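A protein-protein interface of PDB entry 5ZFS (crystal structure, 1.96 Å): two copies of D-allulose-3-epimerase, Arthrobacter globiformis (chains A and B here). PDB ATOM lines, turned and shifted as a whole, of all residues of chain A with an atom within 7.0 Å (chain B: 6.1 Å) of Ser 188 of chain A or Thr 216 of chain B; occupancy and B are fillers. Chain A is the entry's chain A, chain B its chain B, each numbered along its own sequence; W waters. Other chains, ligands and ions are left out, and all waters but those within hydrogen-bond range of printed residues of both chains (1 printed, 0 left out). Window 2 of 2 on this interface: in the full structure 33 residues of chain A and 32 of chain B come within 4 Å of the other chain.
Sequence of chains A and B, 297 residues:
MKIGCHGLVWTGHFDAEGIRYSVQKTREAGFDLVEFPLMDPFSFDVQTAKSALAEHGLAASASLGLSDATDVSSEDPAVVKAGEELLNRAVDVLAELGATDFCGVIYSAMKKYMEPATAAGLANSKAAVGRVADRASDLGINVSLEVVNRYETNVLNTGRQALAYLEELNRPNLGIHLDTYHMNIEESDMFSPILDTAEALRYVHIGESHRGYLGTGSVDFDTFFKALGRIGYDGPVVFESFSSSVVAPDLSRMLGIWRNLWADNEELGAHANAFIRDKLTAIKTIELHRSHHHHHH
No position is printed for both chains.
Of the 8 pairs that touch across the chains among the printed residues, none has its exchanged pair printed and touching as well.
O of Tyr 213 of chain B lies within hydrogen-bond range of OG1 of Thr 216 of chain B, at 2.6 Å.
The backbone NH of Gly 217 of chain B is in hydrogen-bond range of the side-chain carboxylate of Glu 208 of chain B (3.1 Å).
OD2 of Asp 189 of chain A sits at hydrogen-bond distance from OG of Ser 188 of chain A (2.9 Å).
A ring nitrogen (ND1) of His 210 of chain B lies within hydrogen-bond range of the backbone NH (N) of Gly 212 of chain B (2.9 Å).
NE2 of His 210 of chain B is in hydrogen-bond range of O of Thr 216 of chain B.
The backbone NH (N) of Ser 218 of chain B sits at hydrogen-bond distance from the side-chain hydroxyl (OG) of Ser 209 of chain B (3.1 Å).
Hydrophobic or aromatic side chains of chain A that line the printed part of chain B: Ile 185.
Of the 11 printed residues of chain B, 4 touch a printed residue of chain A.
Among the printed residues, 8 pairs touch across the chains.
Among the printed residues, no Asp or Glu carboxylate lies within 4 Å of a Lys or Arg side-chain nitrogen of the other chain.
Water W1 lies within hydrogen-bond range of the backbone carbonyl oxygen of Glu 187 of chain A (2.6 Å), the side-chain hydroxyl of Ser 218 of chain B (2.8 Å), the backbone carbonyl oxygen of Met 183 of chain A (2.9 Å) and the side-chain hydroxyl of Ser 209 of chain B (3.3 Å).
CB of His 210 of chain B touches O of Glu 186 of chain A, at 3.7 Å.
Glu 187 of chain A touches Ser 209 of chain B.
CD2 of His 210 of chain B touches O of Glu 187 of chain A (3.9 Å).
Gly 217 of chain B touches Glu 187 of chain A (CA to O, 3.96 Å).
O of Ser 188 of chain A sits close to O of Gly 217 of chain B, at 3.4 Å.
The backbone carbonyl oxygen (O) of Ile 185 of chain A sits at hydrogen-bond distance from the backbone NH (N) of His 210 of chain B (3.3 Å).
O of Ser 188 of chain A sits close to O of Thr 216 of chain B (3.3 Å).
The backbone carbonyl oxygen (O) of Ile 185 of chain A sits close to the side-chain hydroxyl (OG) of Ser 209 of chain B (3.1 Å).
Of the printed residues of chain B, Ile 185 of chain A touches Ser 209 and His 210.
Printed residues of chain B within 4 Å of Glu 187 of chain A: Ser 209 (3.8 Å), His 210 (3.9 Å) and Gly 217 (3.96 Å).
Printed residues of chain A within 4 Å of Ser 209 of chain B: Ile 185 (3.0 Å) and Glu 187 (3.8 Å).
Thr 216 of chain B touches just one residue of chain A: Ser 188 (3.1 Å).
The nearest residue of chain A that does not touch Thr 216 of chain B is Glu 187 of chain A (4.5 Å).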
ATOM      1  N   THR A 158       0.912   9.743  19.676  1.00  0.00           N
ATOM      2  CA  THR A 158      -0.320  10.427  20.085  1.00  0.00           C
ATOM      3  C   THR A 158      -1.577   9.649  19.684  1.00  0.00           C
ATOM      4  O   THR A 158      -1.564   8.866  18.738  1.00  0.00           O
ATOM      5  CB  THR A 158      -0.436  11.839  19.471  1.00  0.00           C
ATOM      6  OG1 THR A 158      -0.673  11.737  18.062  1.00  0.00           O
ATOM      7  CG2 THR A 158       0.816  12.664  19.722  1.00  0.00           C
ATOM      8  N   MET A 183       0.527   9.702  27.955  1.00  0.00           N
ATOM      9  CA  MET A 183      -0.188  10.929  27.615  1.00  0.00           C
ATOM     10  C   MET A 183       0.502  12.120  28.269  1.00  0.00           C
ATOM     11  O   MET A 183       0.588  13.210  27.695  1.00  0.00           O
ATOM     12  CB  MET A 183      -1.629  10.853  28.116  1.00  0.00           C
ATOM     13  CG  MET A 183      -2.480   9.813  27.406  1.00  0.00           C
ATOM     14  SD  MET A 183      -4.118   9.701  28.136  1.00  0.00           S
ATOM     15  CE  MET A 183      -4.801  11.302  27.740  1.00  0.00           C
ATOM     16  N   ILE A 185       3.362  12.818  28.787  1.00  0.00           N
ATOM     17  CA  ILE A 185       4.451  13.334  27.982  1.00  0.00           C
ATOM     18  C   ILE A 185       3.948  13.966  26.686  1.00  0.00           C
ATOM     19  O   ILE A 185       4.180  15.145  26.440  1.00  0.00           O
ATOM     20  CB  ILE A 185       5.473  12.228  27.669  1.00  0.00           C
ATOM     21  CG1 ILE A 185       6.114  11.731  28.967  1.00  0.00           C
ATOM     22  CG2 ILE A 185       6.533  12.745  26.705  1.00  0.00           C
ATOM     23  CD1 ILE A 185       6.670  10.324  28.882  1.00  0.00           C
ATOM     24  N   GLU A 186       3.252  13.191  25.859  1.00  0.00           N
ATOM     25  CA  GLU A 186       3.151  13.513  24.439  1.00  0.00           C
ATOM     26  C   GLU A 186       1.951  14.388  24.084  1.00  0.00           C
ATOM     27  O   GLU A 186       1.983  15.090  23.080  1.00  0.00           O
ATOM     28  CB  GLU A 186       3.134  12.233  23.591  1.00  0.00           C
ATOM     29  CG  GLU A 186       4.351  11.338  23.774  1.00  0.00           C
ATOM     30  CD  GLU A 186       5.632  11.908  23.195  1.00  0.00           C
ATOM     31  OE1 GLU A 186       5.577  12.887  22.418  1.00  0.00           O
ATOM     32  OE2 GLU A 186       6.712  11.373  23.518  1.00  0.00           O
ATOM     33  N   GLU A 187       0.893  14.349  24.886  1.00  0.00           N
ATOM     34  CA  GLU A 187      -0.383  14.930  24.466  1.00  0.00           C
ATOM     35  C   GLU A 187      -0.499  16.388  24.901  1.00  0.00           C
ATOM     36  O   GLU A 187       0.224  16.838  25.787  1.00  0.00           O
ATOM     37  CB  GLU A 187      -1.566  14.116  24.993  1.00  0.00           C
ATOM     38  CG  GLU A 187      -1.494  12.637  24.644  1.00  0.00           C
ATOM     39  CD  GLU A 187      -2.048  12.306  23.265  1.00  0.00           C
ATOM     40  OE1 GLU A 187      -2.373  13.236  22.488  1.00  0.00           O
ATOM     41  OE2 GLU A 187      -2.170  11.100  22.956  1.00  0.00           O
ATOM     42  N   SER A 188      -1.401  17.125  24.258  1.00  0.00           N
ATOM     43  CA  SER A 188      -1.589  18.541  24.555  1.00  0.00           C
ATOM     44  C   SER A 188      -2.213  18.747  25.933  1.00  0.00           C
ATOM     45  O   SER A 188      -1.961  19.758  26.590  1.00  0.00           O
ATOM     46  CB  SER A 188      -2.450  19.208  23.479  1.00  0.00           C
ATOM     47  OG  SER A 188      -3.760  18.661  23.447  1.00  0.00           O
ATOM     48  N   ASP A 189      -3.009  17.776  26.366  1.00  0.00           N
ATOM     49  CA  ASP A 189      -3.732  17.843  27.628  1.00  0.00           C
ATOM     50  C   ASP A 189      -4.390  16.489  27.840  1.00  0.00           C
ATOM     51  O   ASP A 189      -4.274  15.611  26.990  1.00  0.00           O
ATOM     52  CB  ASP A 189      -4.809  18.930  27.583  1.00  0.00           C
ATOM     53  CG  ASP A 189      -5.820  18.698  26.475  1.00  0.00           C
ATOM     54  OD1 ASP A 189      -6.655  17.782  26.615  1.00  0.00           O
ATOM     55  OD2 ASP A 189      -5.771  19.429  25.459  1.00  0.00           O
ATOM     56  N   MET A 190      -5.078  16.319  28.967  1.00  0.00           N
ATOM     57  CA  MET A 190      -5.574  15.004  29.346  1.00  0.00           C
ATOM     58  C   MET A 190      -7.043  14.778  28.987  1.00  0.00           C
ATOM     59  O   MET A 190      -7.579  13.702  29.263  1.00  0.00           O
ATOM     60  CB  MET A 190      -5.366  14.753  30.842  1.00  0.00           C
ATOM     61  CG  MET A 190      -3.914  14.814  31.296  1.00  0.00           C
ATOM     62  SD  MET A 190      -2.839  13.544  30.583  1.00  0.00           S
ATOM     63  CE  MET A 190      -3.415  12.082  31.433  1.00  0.00           C
ATOM     64  N   PHE A 191      -7.697  15.761  28.368  1.00  0.00           N
ATOM     65  CA  PHE A 191      -9.076  15.562  27.918  1.00  0.00           C
ATOM     66  C   PHE A 191      -9.253  15.474  26.394  1.00  0.00           C
ATOM     67  O   PHE A 191     -10.063  14.675  25.909  1.00  0.00           O
ATOM     68  CB  PHE A 191     -10.033  16.594  28.536  1.00  0.00           C
ATOM     69  CG  PHE A 191      -9.881  17.991  27.997  1.00  0.00           C
ATOM     70  CD1 PHE A 191      -8.986  18.878  28.573  1.00  0.00           C
ATOM     71  CD2 PHE A 191     -10.658  18.427  26.939  1.00  0.00           C
ATOM     72  CE1 PHE A 191      -8.856  20.169  28.088  1.00  0.00           C
ATOM     73  CE2 PHE A 191     -10.533  19.718  26.449  1.00  0.00           C
ATOM     74  CZ  PHE A 191      -9.629  20.589  27.025  1.00  0.00           C
ATOM     75  N   SER A 192      -8.496  16.277  25.648  1.00  0.00           N
ATOM     76  CA  SER A 192      -8.619  16.328  24.187  1.00  0.00           C
ATOM     77  C   SER A 192      -8.467  14.952  23.534  1.00  0.00           C
ATOM     78  O   SER A 192      -9.231  14.603  22.634  1.00  0.00           O
ATOM     79  CB  SER A 192      -7.571  17.277  23.598  1.00  0.00           C
ATOM     80  OG  SER A 192      -7.792  18.597  24.045  1.00  0.00           O
ATOM     81  N   PRO A 193      -7.470  14.173  23.976  1.00  0.00           N
ATOM     82  CA  PRO A 193      -7.207  12.864  23.373  1.00  0.00           C
ATOM     83  C   PRO A 193      -8.333  11.868  23.619  1.00  0.00           C
ATOM     84  O   PRO A 193      -8.569  10.987  22.796  1.00  0.00           O
ATOM     85  CB  PRO A 193      -5.921  12.401  24.067  1.00  0.00           C
ATOM     86  CG  PRO A 193      -5.316  13.633  24.646  1.00  0.00           C
ATOM     87  CD  PRO A 193      -6.479  14.505  25.011  1.00  0.00           C
ATOM     88  N   GLU B 208       8.169  22.288  27.471  1.00  0.00           N
ATOM     89  CA  GLU B 208       6.823  21.745  27.582  1.00  0.00           C
ATOM     90  C   GLU B 208       6.895  20.218  27.574  1.00  0.00           C
ATOM     91  O   GLU B 208       7.935  19.644  27.254  1.00  0.00           O
ATOM     92  CB  GLU B 208       5.959  22.283  26.433  1.00  0.00           C
ATOM     93  CG  GLU B 208       4.471  21.979  26.505  1.00  0.00           C
ATOM     94  CD  GLU B 208       3.844  22.289  27.852  1.00  0.00           C
ATOM     95  OE1 GLU B 208       3.922  21.424  28.742  1.00  0.00           O
ATOM     96  OE2 GLU B 208       3.248  23.382  28.012  1.00  0.00           O
ATOM     97  N   SER B 209       5.800  19.564  27.952  1.00  0.00           N
ATOM     98  CA  SER B 209       5.806  18.116  28.169  1.00  0.00           C
ATOM     99  C   SER B 209       6.263  17.332  26.935  1.00  0.00           C
ATOM    100  O   SER B 209       6.910  16.281  27.062  1.00  0.00           O
ATOM    101  CB  SER B 209       4.417  17.642  28.599  1.00  0.00           C
ATOM    102  OG  SER B 209       3.444  17.896  27.592  1.00  0.00           O
ATOM    103  N   HIS B 210       5.919  17.845  25.751  1.00  0.00           N
ATOM    104  CA  HIS B 210       6.294  17.224  24.484  1.00  0.00           C
ATOM    105  C   HIS B 210       7.401  18.020  23.772  1.00  0.00           C
ATOM    106  O   HIS B 210       7.742  17.725  22.625  1.00  0.00           O
ATOM    107  CB  HIS B 210       5.064  17.133  23.575  1.00  0.00           C
ATOM    108  CG  HIS B 210       4.286  18.411  23.492  1.00  0.00           C
ATOM    109  ND1 HIS B 210       4.883  19.633  23.270  1.00  0.00           N
ATOM    110  CD2 HIS B 210       2.962  18.660  23.631  1.00  0.00           C
ATOM    111  CE1 HIS B 210       3.958  20.576  23.256  1.00  0.00           C
ATOM    112  NE2 HIS B 210       2.784  20.012  23.470  1.00  0.00           N
ATOM    113  N   GLY B 212       7.349  21.026  22.661  1.00  0.00           N
ATOM    114  CA  GLY B 212       6.838  21.947  21.642  1.00  0.00           C
ATOM    115  C   GLY B 212       6.625  23.364  22.163  1.00  0.00           C
ATOM    116  O   GLY B 212       7.350  23.822  23.045  1.00  0.00           O
ATOM    117  N   TYR B 213       5.629  24.054  21.611  1.00  0.00           N
ATOM    118  CA  TYR B 213       5.221  25.370  22.107  1.00  0.00           C
ATOM    119  C   TYR B 213       4.908  25.316  23.597  1.00  0.00           C
ATOM    120  O   TYR B 213       4.173  24.443  24.049  1.00  0.00           O
ATOM    121  CB  TYR B 213       3.977  25.859  21.368  1.00  0.00           C
ATOM    122  CG  TYR B 213       4.254  26.682  20.124  1.00  0.00           C
ATOM    123  CD1 TYR B 213       4.435  26.067  18.893  1.00  0.00           C
ATOM    124  CD2 TYR B 213       4.316  28.070  20.180  1.00  0.00           C
ATOM    125  CE1 TYR B 213       4.677  26.810  17.750  1.00  0.00           C
ATOM    126  CE2 TYR B 213       4.558  28.820  19.040  1.00  0.00           C
ATOM    127  CZ  TYR B 213       4.745  28.183  17.830  1.00  0.00           C
ATOM    128  OH  TYR B 213       4.990  28.913  16.690  1.00  0.00           O
ATOM    129  N   LEU B 214       5.437  26.282  24.346  1.00  0.00           N
ATOM    130  CA  LEU B 214       5.079  26.452  25.746  1.00  0.00           C
ATOM    131  C   LEU B 214       3.594  26.728  25.921  1.00  0.00           C
ATOM    132  O   LEU B 214       3.007  27.564  25.218  1.00  0.00           O
ATOM    133  CB  LEU B 214       5.894  27.587  26.377  1.00  0.00           C
ATOM    134  CG  LEU B 214       7.417  27.438  26.329  1.00  0.00           C
ATOM    135  CD1 LEU B 214       8.093  28.556  27.110  1.00  0.00           C
ATOM    136  CD2 LEU B 214       7.858  26.085  26.863  1.00  0.00           C
ATOM    137  N   GLY B 215       2.988  26.026  26.876  1.00  0.00           N
ATOM    138  CA  GLY B 215       1.574  26.179  27.154  1.00  0.00           C
ATOM    139  C   GLY B 215       0.704  25.264  26.306  1.00  0.00           C
ATOM    140  O   GLY B 215      -0.511  25.372  26.352  1.00  0.00           O
ATOM    141  N   THR B 216       1.310  24.376  25.520  1.00  0.00           N
ATOM    142  CA  THR B 216       0.518  23.453  24.690  1.00  0.00           C
ATOM    143  C   THR B 216       0.621  22.007  25.158  1.00  0.00           C
ATOM    144  O   THR B 216       0.221  21.092  24.445  1.00  0.00           O
ATOM    145  CB  THR B 216       0.898  23.520  23.201  1.00  0.00           C
ATOM    146  OG1 THR B 216       2.242  23.056  23.005  1.00  0.00           O
ATOM    147  CG2 THR B 216       0.757  24.942  22.670  1.00  0.00           C
ATOM    148  N   GLY B 217       1.143  21.809  26.364  1.00  0.00           N
ATOM    149  CA  GLY B 217       1.227  20.483  26.959  1.00  0.00           C
ATOM    150  C   GLY B 217       0.810  20.510  28.411  1.00  0.00           C
ATOM    151  O   GLY B 217       0.054  21.380  28.829  1.00  0.00           O
ATOM    152  N   SER B 218       1.303  19.554  29.192  1.00  0.00           N
ATOM    153  CA  SER B 218       0.775  19.340  30.532  1.00  0.00           C
ATOM    154  C   SER B 218       1.759  19.712  31.648  1.00  0.00           C
ATOM    155  O   SER B 218       1.528  19.382  32.808  1.00  0.00           O
ATOM    156  CB  SER B 218       0.331  17.884  30.694  1.00  0.00           C
ATOM    157  OG  SER B 218       1.440  17.005  30.652  1.00  0.00           O
ATOM    158  N   LEU B 261       6.374  19.482  15.757  1.00  0.00           N
ATOM    159  CA  LEU B 261       5.646  20.216  16.794  1.00  0.00           C
ATOM    160  C   LEU B 261       5.600  21.716  16.485  1.00  0.00           C
ATOM    161  O   LEU B 261       4.835  22.472  17.101  1.00  0.00           O
ATOM    162  CB  LEU B 261       6.291  19.967  18.155  1.00  0.00           C
ATOM    163  CG  LEU B 261       5.826  18.678  18.839  1.00  0.00           C
ATOM    164  CD1 LEU B 261       6.907  18.156  19.757  1.00  0.00           C
ATOM    165  CD2 LEU B 261       4.533  18.902  19.607  1.00  0.00           C
HETATM  166  O   HOH W   1       0.746  16.022  28.162  1.00  0.00           O
